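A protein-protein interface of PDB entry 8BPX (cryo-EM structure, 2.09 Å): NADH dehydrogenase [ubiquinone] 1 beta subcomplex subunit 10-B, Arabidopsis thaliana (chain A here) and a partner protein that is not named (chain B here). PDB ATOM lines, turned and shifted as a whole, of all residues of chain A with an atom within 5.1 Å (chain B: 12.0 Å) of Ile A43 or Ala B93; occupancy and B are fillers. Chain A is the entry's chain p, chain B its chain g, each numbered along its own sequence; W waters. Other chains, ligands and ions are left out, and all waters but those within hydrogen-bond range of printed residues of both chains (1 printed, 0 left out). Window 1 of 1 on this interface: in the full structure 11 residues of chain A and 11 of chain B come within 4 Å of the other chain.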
ATOM      1  N   ARG A  39      19.881 -27.784   9.785  1.00  0.00           N
ATOM      2  CA  ARG A  39      19.211 -28.595  10.797  1.00  0.00           C
ATOM      3  C   ARG A  39      19.615 -28.174  12.208  1.00  0.00           C
ATOM      4  O   ARG A  39      18.767 -28.090  13.109  1.00  0.00           O
ATOM      5  CB  ARG A  39      19.511 -30.073  10.548  1.00  0.00           C
ATOM      6  CG  ARG A  39      18.310 -30.860  10.053  1.00  0.00           C
ATOM      7  CD  ARG A  39      18.573 -31.651   8.794  1.00  0.00           C
ATOM      8  NE  ARG A  39      19.823 -32.399   8.821  1.00  0.00           N
ATOM      9  CZ  ARG A  39      20.409 -32.899   7.740  1.00  0.00           C
ATOM     10  NH1 ARG A  39      19.882 -32.749   6.538  1.00  0.00           N
ATOM     11  NH2 ARG A  39      21.551 -33.565   7.870  1.00  0.00           N
ATOM     12  N   GLU A  40      20.899 -27.879  12.413  1.00  0.00           N
ATOM     13  CA  GLU A  40      21.445 -27.444  13.731  1.00  0.00           C
ATOM     14  C   GLU A  40      20.821 -26.120  14.120  1.00  0.00           C
ATOM     15  O   GLU A  40      20.320 -26.014  15.213  1.00  0.00           O
ATOM     16  CB  GLU A  40      22.982 -27.401  13.704  1.00  0.00           C
ATOM     17  CG  GLU A  40      23.629 -28.766  13.737  1.00  0.00           C
ATOM     18  CD  GLU A  40      23.289 -29.569  14.974  1.00  0.00           C
ATOM     19  OE1 GLU A  40      23.584 -29.100  16.070  1.00  0.00           O
ATOM     20  OE2 GLU A  40      22.719 -30.646  14.840  1.00  0.00           O
ATOM     21  N   LYS A  41      20.759 -25.193  13.180  1.00  0.00           N
ATOM     22  CA  LYS A  41      20.099 -23.904  13.399  1.00  0.00           C
ATOM     23  C   LYS A  41      18.625 -24.074  13.811  1.00  0.00           C
ATOM     24  O   LYS A  41      18.236 -23.379  14.718  1.00  0.00           O
ATOM     25  CB  LYS A  41      20.383 -22.918  12.251  1.00  0.00           C
ATOM     26  CG  LYS A  41      21.805 -22.405  12.163  1.00  0.00           C
ATOM     27  CD  LYS A  41      22.021 -21.452  11.029  1.00  0.00           C
ATOM     28  CE  LYS A  41      23.424 -20.896  11.016  1.00  0.00           C
ATOM     29  NZ  LYS A  41      23.515 -19.601  10.313  1.00  0.00           N
ATOM     30  N   TRP A  42      17.884 -24.993  13.200  1.00  0.00           N
ATOM     31  CA  TRP A  42      16.496 -25.278  13.597  1.00  0.00           C
ATOM     32  C   TRP A  42      16.432 -25.871  15.033  1.00  0.00           C
ATOM     33  O   TRP A  42      15.499 -25.550  15.711  1.00  0.00           O
ATOM     34  CB  TRP A  42      15.738 -26.117  12.567  1.00  0.00           C
ATOM     35  CG  TRP A  42      15.226 -25.253  11.461  1.00  0.00           C
ATOM     36  CD1 TRP A  42      15.774 -25.098  10.229  1.00  0.00           C
ATOM     37  CD2 TRP A  42      14.092 -24.379  11.512  1.00  0.00           C
ATOM     38  NE1 TRP A  42      15.039 -24.225   9.495  1.00  0.00           N
ATOM     39  CE2 TRP A  42      14.008 -23.753  10.252  1.00  0.00           C
ATOM     40  CE3 TRP A  42      13.141 -24.069  12.487  1.00  0.00           C
ATOM     41  CZ2 TRP A  42      13.009 -22.835   9.941  1.00  0.00           C
ATOM     42  CZ3 TRP A  42      12.156 -23.160  12.181  1.00  0.00           C
ATOM     43  CH2 TRP A  42      12.086 -22.560  10.923  1.00  0.00           C
ATOM     44  N   ILE A  43      17.419 -26.670  15.399  1.00  0.00           N
ATOM     45  CA  ILE A  43      17.447 -27.202  16.786  1.00  0.00           C
ATOM     46  C   ILE A  43      17.608 -26.034  17.778  1.00  0.00           C
ATOM     47  O   ILE A  43      16.804 -26.020  18.679  1.00  0.00           O
ATOM     48  CB  ILE A  43      18.425 -28.367  16.973  1.00  0.00           C
ATOM     49  CG1 ILE A  43      18.055 -29.570  16.104  1.00  0.00           C
ATOM     50  CG2 ILE A  43      18.574 -28.747  18.442  1.00  0.00           C
ATOM     51  CD1 ILE A  43      19.225 -30.455  15.819  1.00  0.00           C
ATOM     52  N   GLN A  44      18.456 -25.046  17.511  1.00  0.00           N
ATOM     53  CA  GLN A  44      18.602 -23.844  18.368  1.00  0.00           C
ATOM     54  C   GLN A  44      17.301 -23.000  18.401  1.00  0.00           C
ATOM     55  O   GLN A  44      17.004 -22.494  19.441  1.00  0.00           O
ATOM     56  CB  GLN A  44      19.883 -23.066  18.075  1.00  0.00           C
ATOM     57  CG  GLN A  44      21.132 -23.922  18.079  1.00  0.00           C
ATOM     58  CD  GLN A  44      22.192 -23.312  17.204  1.00  0.00           C
ATOM     59  OE1 GLN A  44      22.844 -22.345  17.582  1.00  0.00           O
ATOM     60  NE2 GLN A  44      22.361 -23.860  16.011  1.00  0.00           N
ATOM     61  N   ILE A  45      16.599 -22.867  17.264  1.00  0.00           N
ATOM     62  CA  ILE A  45      15.324 -22.128  17.214  1.00  0.00           C
ATOM     63  C   ILE A  45      14.310 -22.858  18.109  1.00  0.00           C
ATOM     64  O   ILE A  45      13.757 -22.188  18.967  1.00  0.00           O
ATOM     65  CB  ILE A  45      14.821 -21.843  15.780  1.00  0.00           C
ATOM     66  CG1 ILE A  45      15.776 -20.928  15.009  1.00  0.00           C
ATOM     67  CG2 ILE A  45      13.392 -21.321  15.768  1.00  0.00           C
ATOM     68  CD1 ILE A  45      15.947 -21.327  13.563  1.00  0.00           C
ATOM     69  N   GLU A  46      14.212 -24.148  17.959  1.00  0.00           N
ATOM     70  CA  GLU A  46      13.259 -24.994  18.744  1.00  0.00           C
ATOM     71  C   GLU A  46      13.617 -24.921  20.265  1.00  0.00           C
ATOM     72  O   GLU A  46      12.678 -24.843  21.024  1.00  0.00           O
ATOM     73  CB  GLU A  46      13.041 -26.340  18.072  1.00  0.00           C
ATOM     74  CG  GLU A  46      12.445 -26.280  16.689  1.00  0.00           C
ATOM     75  CD  GLU A  46      11.032 -25.745  16.581  1.00  0.00           C
ATOM     76  OE1 GLU A  46      10.244 -25.944  17.519  1.00  0.00           O
ATOM     77  OE2 GLU A  46      10.737 -25.095  15.565  1.00  0.00           O
ATOM     78  N   LYS A  47      14.890 -24.808  20.640  1.00  0.00           N
ATOM     79  CA  LYS A  47      15.345 -24.624  22.048  1.00  0.00           C
ATOM     80  C   LYS A  47      14.893 -23.268  22.573  1.00  0.00           C
ATOM     81  O   LYS A  47      14.253 -23.268  23.622  1.00  0.00           O
ATOM     82  CB  LYS A  47      16.855 -24.819  22.206  1.00  0.00           C
ATOM     83  CG  LYS A  47      17.364 -26.222  22.436  1.00  0.00           C
ATOM     84  CD  LYS A  47      18.788 -26.136  22.900  1.00  0.00           C
ATOM     85  CE  LYS A  47      19.717 -27.122  22.242  1.00  0.00           C
ATOM     86  NZ  LYS A  47      19.587 -28.467  22.830  1.00  0.00           N
ATOM     87  N   ASP B  86       3.747 -35.819   9.042  1.00  0.00           N
ATOM     88  CA  ASP B  86       4.336 -34.528   9.386  1.00  0.00           C
ATOM     89  C   ASP B  86       5.851 -34.661   9.296  1.00  0.00           C
ATOM     90  O   ASP B  86       6.488 -35.267  10.159  1.00  0.00           O
ATOM     91  CB  ASP B  86       3.886 -34.087  10.774  1.00  0.00           C
ATOM     92  CG  ASP B  86       4.469 -32.752  11.181  1.00  0.00           C
ATOM     93  OD1 ASP B  86       4.526 -32.478  12.395  1.00  0.00           O
ATOM     94  OD2 ASP B  86       4.863 -31.967  10.294  1.00  0.00           O
ATOM     95  N   LEU B  87       6.423 -34.034   8.277  1.00  0.00           N
ATOM     96  CA  LEU B  87       7.870 -34.152   7.996  1.00  0.00           C
ATOM     97  C   LEU B  87       8.541 -32.790   8.162  1.00  0.00           C
ATOM     98  O   LEU B  87       9.718 -32.695   7.911  1.00  0.00           O
ATOM     99  CB  LEU B  87       8.060 -34.726   6.591  1.00  0.00           C
ATOM    100  CG  LEU B  87       7.490 -36.123   6.369  1.00  0.00           C
ATOM    101  CD1 LEU B  87       7.742 -36.580   4.943  1.00  0.00           C
ATOM    102  CD2 LEU B  87       8.077 -37.113   7.363  1.00  0.00           C
ATOM    103  N   SER B  88       7.825 -31.797   8.668  1.00  0.00           N
ATOM    104  CA  SER B  88       8.352 -30.445   8.738  1.00  0.00           C
ATOM    105  C   SER B  88       9.633 -30.405   9.567  1.00  0.00           C
ATOM    106  O   SER B  88       9.813 -31.175  10.515  1.00  0.00           O
ATOM    107  CB  SER B  88       7.302 -29.503   9.325  1.00  0.00           C
ATOM    108  OG  SER B  88       7.111 -29.747  10.704  1.00  0.00           O
ATOM    109  N   ILE B  89      10.538 -29.502   9.184  1.00  0.00           N
ATOM    110  CA  ILE B  89      11.796 -29.350   9.909  1.00  0.00           C
ATOM    111  C   ILE B  89      11.531 -28.909  11.344  1.00  0.00           C
ATOM    112  O   ILE B  89      12.242 -29.317  12.267  1.00  0.00           O
ATOM    113  CB  ILE B  89      12.730 -28.370   9.168  1.00  0.00           C
ATOM    114  CG1 ILE B  89      13.994 -28.107   9.982  1.00  0.00           C
ATOM    115  CG2 ILE B  89      12.035 -27.053   8.890  1.00  0.00           C
ATOM    116  CD1 ILE B  89      14.995 -29.215   9.907  1.00  0.00           C
ATOM    117  N   GLU B  90      10.498 -28.091  11.554  1.00  0.00           N
ATOM    118  CA  GLU B  90      10.153 -27.644  12.898  1.00  0.00           C
ATOM    119  C   GLU B  90       9.813 -28.827  13.801  1.00  0.00           C
ATOM    120  O   GLU B  90      10.293 -28.910  14.937  1.00  0.00           O
ATOM    121  CB  GLU B  90       8.982 -26.665  12.836  1.00  0.00           C
ATOM    122  CG  GLU B  90       9.283 -25.371  12.114  1.00  0.00           C
ATOM    123  CD  GLU B  90       8.817 -25.372  10.664  1.00  0.00           C
ATOM    124  OE1 GLU B  90       8.618 -24.277  10.111  1.00  0.00           O
ATOM    125  OE2 GLU B  90       8.667 -26.463  10.071  1.00  0.00           O
ATOM    126  N   THR B  91       8.999 -29.759  13.306  1.00  0.00           N
ATOM    127  CA  THR B  91       8.604 -30.910  14.113  1.00  0.00           C
ATOM    128  C   THR B  91       9.791 -31.811  14.429  1.00  0.00           C
ATOM    129  O   THR B  91       9.927 -32.287  15.560  1.00  0.00           O
ATOM    130  CB  THR B  91       7.509 -31.702  13.399  1.00  0.00           C
ATOM    131  OG1 THR B  91       6.364 -30.865  13.209  1.00  0.00           O
ATOM    132  CG2 THR B  91       7.112 -32.923  14.210  1.00  0.00           C
ATOM    133  N   TRP B  92      10.651 -32.068  13.439  1.00  0.00           N
ATOM    134  CA  TRP B  92      11.834 -32.884  13.690  1.00  0.00           C
ATOM    135  C   TRP B  92      12.787 -32.197  14.661  1.00  0.00           C
ATOM    136  O   TRP B  92      13.349 -32.844  15.550  1.00  0.00           O
ATOM    137  CB  TRP B  92      12.547 -33.207  12.376  1.00  0.00           C
ATOM    138  CG  TRP B  92      13.886 -33.853  12.568  1.00  0.00           C
ATOM    139  CD1 TRP B  92      14.150 -35.184  12.605  1.00  0.00           C
ATOM    140  CD2 TRP B  92      15.146 -33.191  12.737  1.00  0.00           C
ATOM    141  NE1 TRP B  92      15.490 -35.399  12.799  1.00  0.00           N
ATOM    142  CE2 TRP B  92      16.125 -34.188  12.885  1.00  0.00           C
ATOM    143  CE3 TRP B  92      15.538 -31.851  12.787  1.00  0.00           C
ATOM    144  CZ2 TRP B  92      17.472 -33.891  13.072  1.00  0.00           C
ATOM    145  CZ3 TRP B  92      16.871 -31.558  12.981  1.00  0.00           C
ATOM    146  CH2 TRP B  92      17.824 -32.573  13.115  1.00  0.00           C
ATOM    147  N   ALA B  93      12.986 -30.889  14.501  1.00  0.00           N
ATOM    148  CA  ALA B  93      13.909 -30.178  15.379  1.00  0.00           C
ATOM    149  C   ALA B  93      13.352 -30.042  16.791  1.00  0.00           C
ATOM    150  O   ALA B  93      14.122 -30.041  17.754  1.00  0.00           O
ATOM    151  CB  ALA B  93      14.246 -28.808  14.798  1.00  0.00           C
ATOM    152  N   HIS B  94      12.049 -29.875  16.937  1.00  0.00           N
ATOM    153  CA  HIS B  94      11.403 -29.823  18.282  1.00  0.00           C
ATOM    154  C   HIS B  94      11.697 -31.104  19.107  1.00  0.00           C
ATOM    155  O   HIS B  94      12.141 -30.978  20.207  1.00  0.00           O
ATOM    156  CB  HIS B  94       9.919 -29.443  18.188  1.00  0.00           C
ATOM    157  CG  HIS B  94       9.279 -29.292  19.525  1.00  0.00           C
ATOM    158  ND1 HIS B  94       9.168 -28.081  20.152  1.00  0.00           N
ATOM    159  CD2 HIS B  94       8.763 -30.199  20.373  1.00  0.00           C
ATOM    160  CE1 HIS B  94       8.584 -28.241  21.308  1.00  0.00           C
ATOM    161  NE2 HIS B  94       8.332 -29.523  21.472  1.00  0.00           N
ATOM    162  N   GLN B  95      11.515 -32.276  18.500  1.00  0.00           N
ATOM    163  CA  GLN B  95      11.825 -33.514  19.207  1.00  0.00           C
ATOM    164  C   GLN B  95      13.312 -33.621  19.505  1.00  0.00           C
ATOM    165  O   GLN B  95      13.710 -34.117  20.564  1.00  0.00           O
ATOM    166  CB  GLN B  95      11.353 -34.725  18.397  1.00  0.00           C
ATOM    167  CG  GLN B  95      11.473 -36.106  19.064  1.00  0.00           C
ATOM    168  CD  GLN B  95      10.840 -37.264  18.291  1.00  0.00           C
ATOM    169  OE1 GLN B  95      10.198 -37.071  17.257  1.00  0.00           O
ATOM    170  NE2 GLN B  95      11.043 -38.480  18.791  1.00  0.00           N
ATOM    171  N   LYS B  96      14.150 -33.165  18.574  1.00  0.00           N
ATOM    172  CA  LYS B  96      15.589 -33.149  18.795  1.00  0.00           C
ATOM    173  C   LYS B  96      15.972 -32.169  19.903  1.00  0.00           C
ATOM    174  O   LYS B  96      16.859 -32.457  20.713  1.00  0.00           O
ATOM    175  CB  LYS B  96      16.294 -32.797  17.485  1.00  0.00           C
ATOM    176  CG  LYS B  96      16.499 -33.950  16.507  1.00  0.00           C
ATOM    177  CD  LYS B  96      17.642 -34.852  16.924  1.00  0.00           C
ATOM    178  CE  LYS B  96      17.493 -36.255  16.356  1.00  0.00           C
ATOM    179  NZ  LYS B  96      16.102 -36.743  16.410  1.00  0.00           N
ATOM    180  N   ALA B  97      15.314 -31.008  19.952  1.00  0.00           N
ATOM    181  CA  ALA B  97      15.606 -30.021  20.988  1.00  0.00           C
ATOM    182  C   ALA B  97      15.232 -30.536  22.374  1.00  0.00           C
ATOM    183  O   ALA B  97      15.973 -30.323  23.344  1.00  0.00           O
ATOM    184  CB  ALA B  97      14.871 -28.717  20.687  1.00  0.00           C
ATOM    185  N   LEU B  98      14.032 -31.113  22.515  1.00  0.00           N
ATOM    186  CA  LEU B  98      13.611 -31.727  23.806  1.00  0.00           C
ATOM    187  C   LEU B  98      14.700 -32.675  24.334  1.00  0.00           C
ATOM    188  O   LEU B  98      15.205 -32.377  25.375  1.00  0.00           O
ATOM    189  CB  LEU B  98      12.290 -32.469  23.686  1.00  0.00           C
ATOM    190  CG  LEU B  98      11.053 -31.586  23.567  1.00  0.00           C
ATOM    191  CD1 LEU B  98       9.874 -32.376  23.061  1.00  0.00           C
ATOM    192  CD2 LEU B  98      10.732 -30.895  24.885  1.00  0.00           C
ATOM    193  N   GLU B  99      15.120 -33.647  23.533  1.00  0.00           N
ATOM    194  CA  GLU B  99      16.027 -34.672  24.034  1.00  0.00           C
ATOM    195  C   GLU B  99      17.407 -34.109  24.351  1.00  0.00           C
ATOM    196  O   GLU B  99      18.113 -34.657  25.202  1.00  0.00           O
ATOM    197  CB  GLU B  99      16.116 -35.823  23.031  1.00  0.00           C
ATOM    198  CG  GLU B  99      17.136 -35.659  21.936  1.00  0.00           C
ATOM    199  CD  GLU B  99      16.731 -36.374  20.664  1.00  0.00           C
ATOM    200  OE1 GLU B  99      15.583 -36.859  20.598  1.00  0.00           O
ATOM    201  OE2 GLU B  99      17.559 -36.451  19.731  1.00  0.00           O
ATOM    202  N   ARG B 100      17.806 -33.019  23.701  1.00  0.00           N
ATOM    203  CA  ARG B 100      19.081 -32.401  24.045  1.00  0.00           C
ATOM    204  C   ARG B 100      18.983 -31.588  25.329  1.00  0.00           C
ATOM    205  O   ARG B 100      19.923 -31.583  26.129  1.00  0.00           O
ATOM    206  CB  ARG B 100      19.573 -31.534  22.894  1.00  0.00           C
ATOM    207  CG  ARG B 100      20.269 -32.314  21.795  1.00  0.00           C
ATOM    208  CD  ARG B 100      20.882 -31.376  20.788  1.00  0.00           C
ATOM    209  NE  ARG B 100      21.134 -32.045  19.520  1.00  0.00           N
ATOM    210  CZ  ARG B 100      21.782 -31.503  18.499  1.00  0.00           C
ATOM    211  NH1 ARG B 100      22.242 -30.265  18.549  1.00  0.00           N
ATOM    212  NH2 ARG B 100      21.956 -32.218  17.391  1.00  0.00           N
ATOM    213  N   LEU B 101      17.864 -30.891  25.551  1.00  0.00           N
ATOM    214  CA  LEU B 101      17.683 -30.254  26.851  1.00  0.00           C
ATOM    215  C   LEU B 101      17.550 -31.278  27.968  1.00  0.00           C
ATOM    216  O   LEU B 101      17.984 -31.020  29.093  1.00  0.00           O
ATOM    217  CB  LEU B 101      16.479 -29.313  26.848  1.00  0.00           C
ATOM    218  CG  LEU B 101      16.908 -27.848  26.855  1.00  0.00           C
ATOM    219  CD1 LEU B 101      17.949 -27.606  25.793  1.00  0.00           C
ATOM    220  CD2 LEU B 101      15.737 -26.897  26.686  1.00  0.00           C
ATOM    221  N   GLU B 102      16.964 -32.439  27.680  1.00  0.00           N
ATOM    222  CA  GLU B 102      16.897 -33.492  28.688  1.00  0.00           C
ATOM    223  C   GLU B 102      18.280 -34.065  28.973  1.00  0.00           C
ATOM    224  O   GLU B 102      18.683 -34.195  30.134  1.00  0.00           O
ATOM    225  CB  GLU B 102      15.935 -34.588  28.231  1.00  0.00           C
ATOM    226  CG  GLU B 102      16.196 -35.946  28.846  1.00  0.00           C
ATOM    227  CD  GLU B 102      14.964 -36.829  28.854  1.00  0.00           C
ATOM    228  OE1 GLU B 102      14.139 -36.691  29.783  1.00  0.00           O
ATOM    229  OE2 GLU B 102      14.819 -37.660  27.933  1.00  0.00           O
ATOM    230  N   MET B 103      19.032 -34.394  27.918  1.00  0.00           N
ATOM    231  CA  MET B 103      20.343 -35.010  28.091  1.00  0.00           C
ATOM    232  C   MET B 103      21.315 -34.082  28.803  1.00  0.00           C
ATOM    233  O   MET B 103      22.229 -34.552  29.491  1.00  0.00           O
ATOM    234  CB  MET B 103      20.906 -35.427  26.733  1.00  0.00           C
ATOM    235  CG  MET B 103      20.124 -36.534  26.046  1.00  0.00           C
ATOM    236  SD  MET B 103      20.071 -38.045  27.026  1.00  0.00           S
ATOM    237  CE  MET B 103      21.793 -38.537  26.983  1.00  0.00           C
ATOM    238  N   GLU B 104      21.140 -32.771  28.655  1.00  0.00           N
ATOM    239  CA  GLU B 104      21.990 -31.811  29.346  1.00  0.00           C
ATOM    240  C   GLU B 104      21.477 -31.439  30.730  1.00  0.00           C
ATOM    241  O   GLU B 104      22.277 -31.033  31.582  1.00  0.00           O
ATOM    242  CB  GLU B 104      22.148 -30.549  28.496  1.00  0.00           C
ATOM    243  CG  GLU B 104      21.315 -29.367  28.930  1.00  0.00           C
ATOM    244  CD  GLU B 104      21.526 -28.162  28.033  1.00  0.00           C
ATOM    245  OE1 GLU B 104      22.682 -27.916  27.631  1.00  0.00           O
ATOM    246  OE2 GLU B 104      20.540 -27.460  27.732  1.00  0.00           O
HETATM  247  O   HOH W   1      21.624 -28.439  20.067  1.00  0.00           O
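The guanidinium group (NH1) of Arg B100 is in salt-bridge range of the side-chain carboxylate (OE1) of Glu A40 (3.1 Å).
NZ of Lys B96 lies within salt-bridge range of OE2 of Glu B99. The side-chain amide nitrogen of Gln A44 sits at hydrogen-bond distance from the backbone carbonyl oxygen of Glu A40, at 3.1 Å.
Among the printed residues, merely in contact across the chains: Arg A39 with Ile B89, Arg A39 with Trp B92, Trp A42 with Ile B89, Trp A42 with Glu B90, Trp A42 with Ala B93, Ile A43 with Trp B92, Ile A43 with Ala B93, Ile A43 with Lys B96, Ile A43 with Ala B97, Ile A43 with Arg B100, Glu A46 with Glu B90, Glu A46 with Ala B93, Glu A46 with His B94, Glu A46 with Ala B97, Lys A47 with Ala B97, Lys A47 with Arg B100 and Lys A47 with Leu B101.
Of the printed residues of chain B, Ile A43 touches Trp B92, Ala B93, Lys B96, Ala B97 and Arg B100. Printed residues of chain A within 4 Å of Ala B93: Trp A42 (3.6 Å), Ile A43 (3.9 Å) and Glu A46 (3.6 Å). Printed residues of chain B within 4 Å of Glu A40: Arg B100. No residue of chain B comes within 4 Å of Gln A44. No residue of chain B comes within 4 Å of Ile A45. Lys A47 touches just these residues of chain B: Ala B97 (3.9 Å), Arg B100 (3.1 Å) and Leu B101 (3.4 Å). Of the printed residues of chain A, Ala B97 touches Ile A43 (3.9 Å), Glu A46 (3.98 Å) and Lys A47 (3.9 Å). Printed residues of chain A within 4 Å of Arg B100: Glu A40, Ile A43 and Lys A47. Of the printed residues of chain A, His B94 touches Glu A46 (3.6 Å). Of the printed residues of chain A, Ile B89 touches Arg A39 (3.7 Å) and Trp A42 (3.4 Å). Glu B99 touches none of the printed residues of chain A. Thr B91 touches none of the printed residues of chain A.
Hydrophobic or aromatic side chains of chain B within 4 Å of the printed part of chain A: Ile B89, Trp B92, Ala B93, His B94, Ala B97 and Leu B101. Of the 9 printed residues of chain A, 6 touch a printed residue of chain B. Hydrophobic or aromatic side chains of chain A within 4 Å of the printed part of chain B: Trp A42 and Ile A43. Among the printed residues, 18 pairs touch across the chains.
Water W1 bridges the guanidinium group of Arg B100 and the side-chain amino group of Lys A47.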
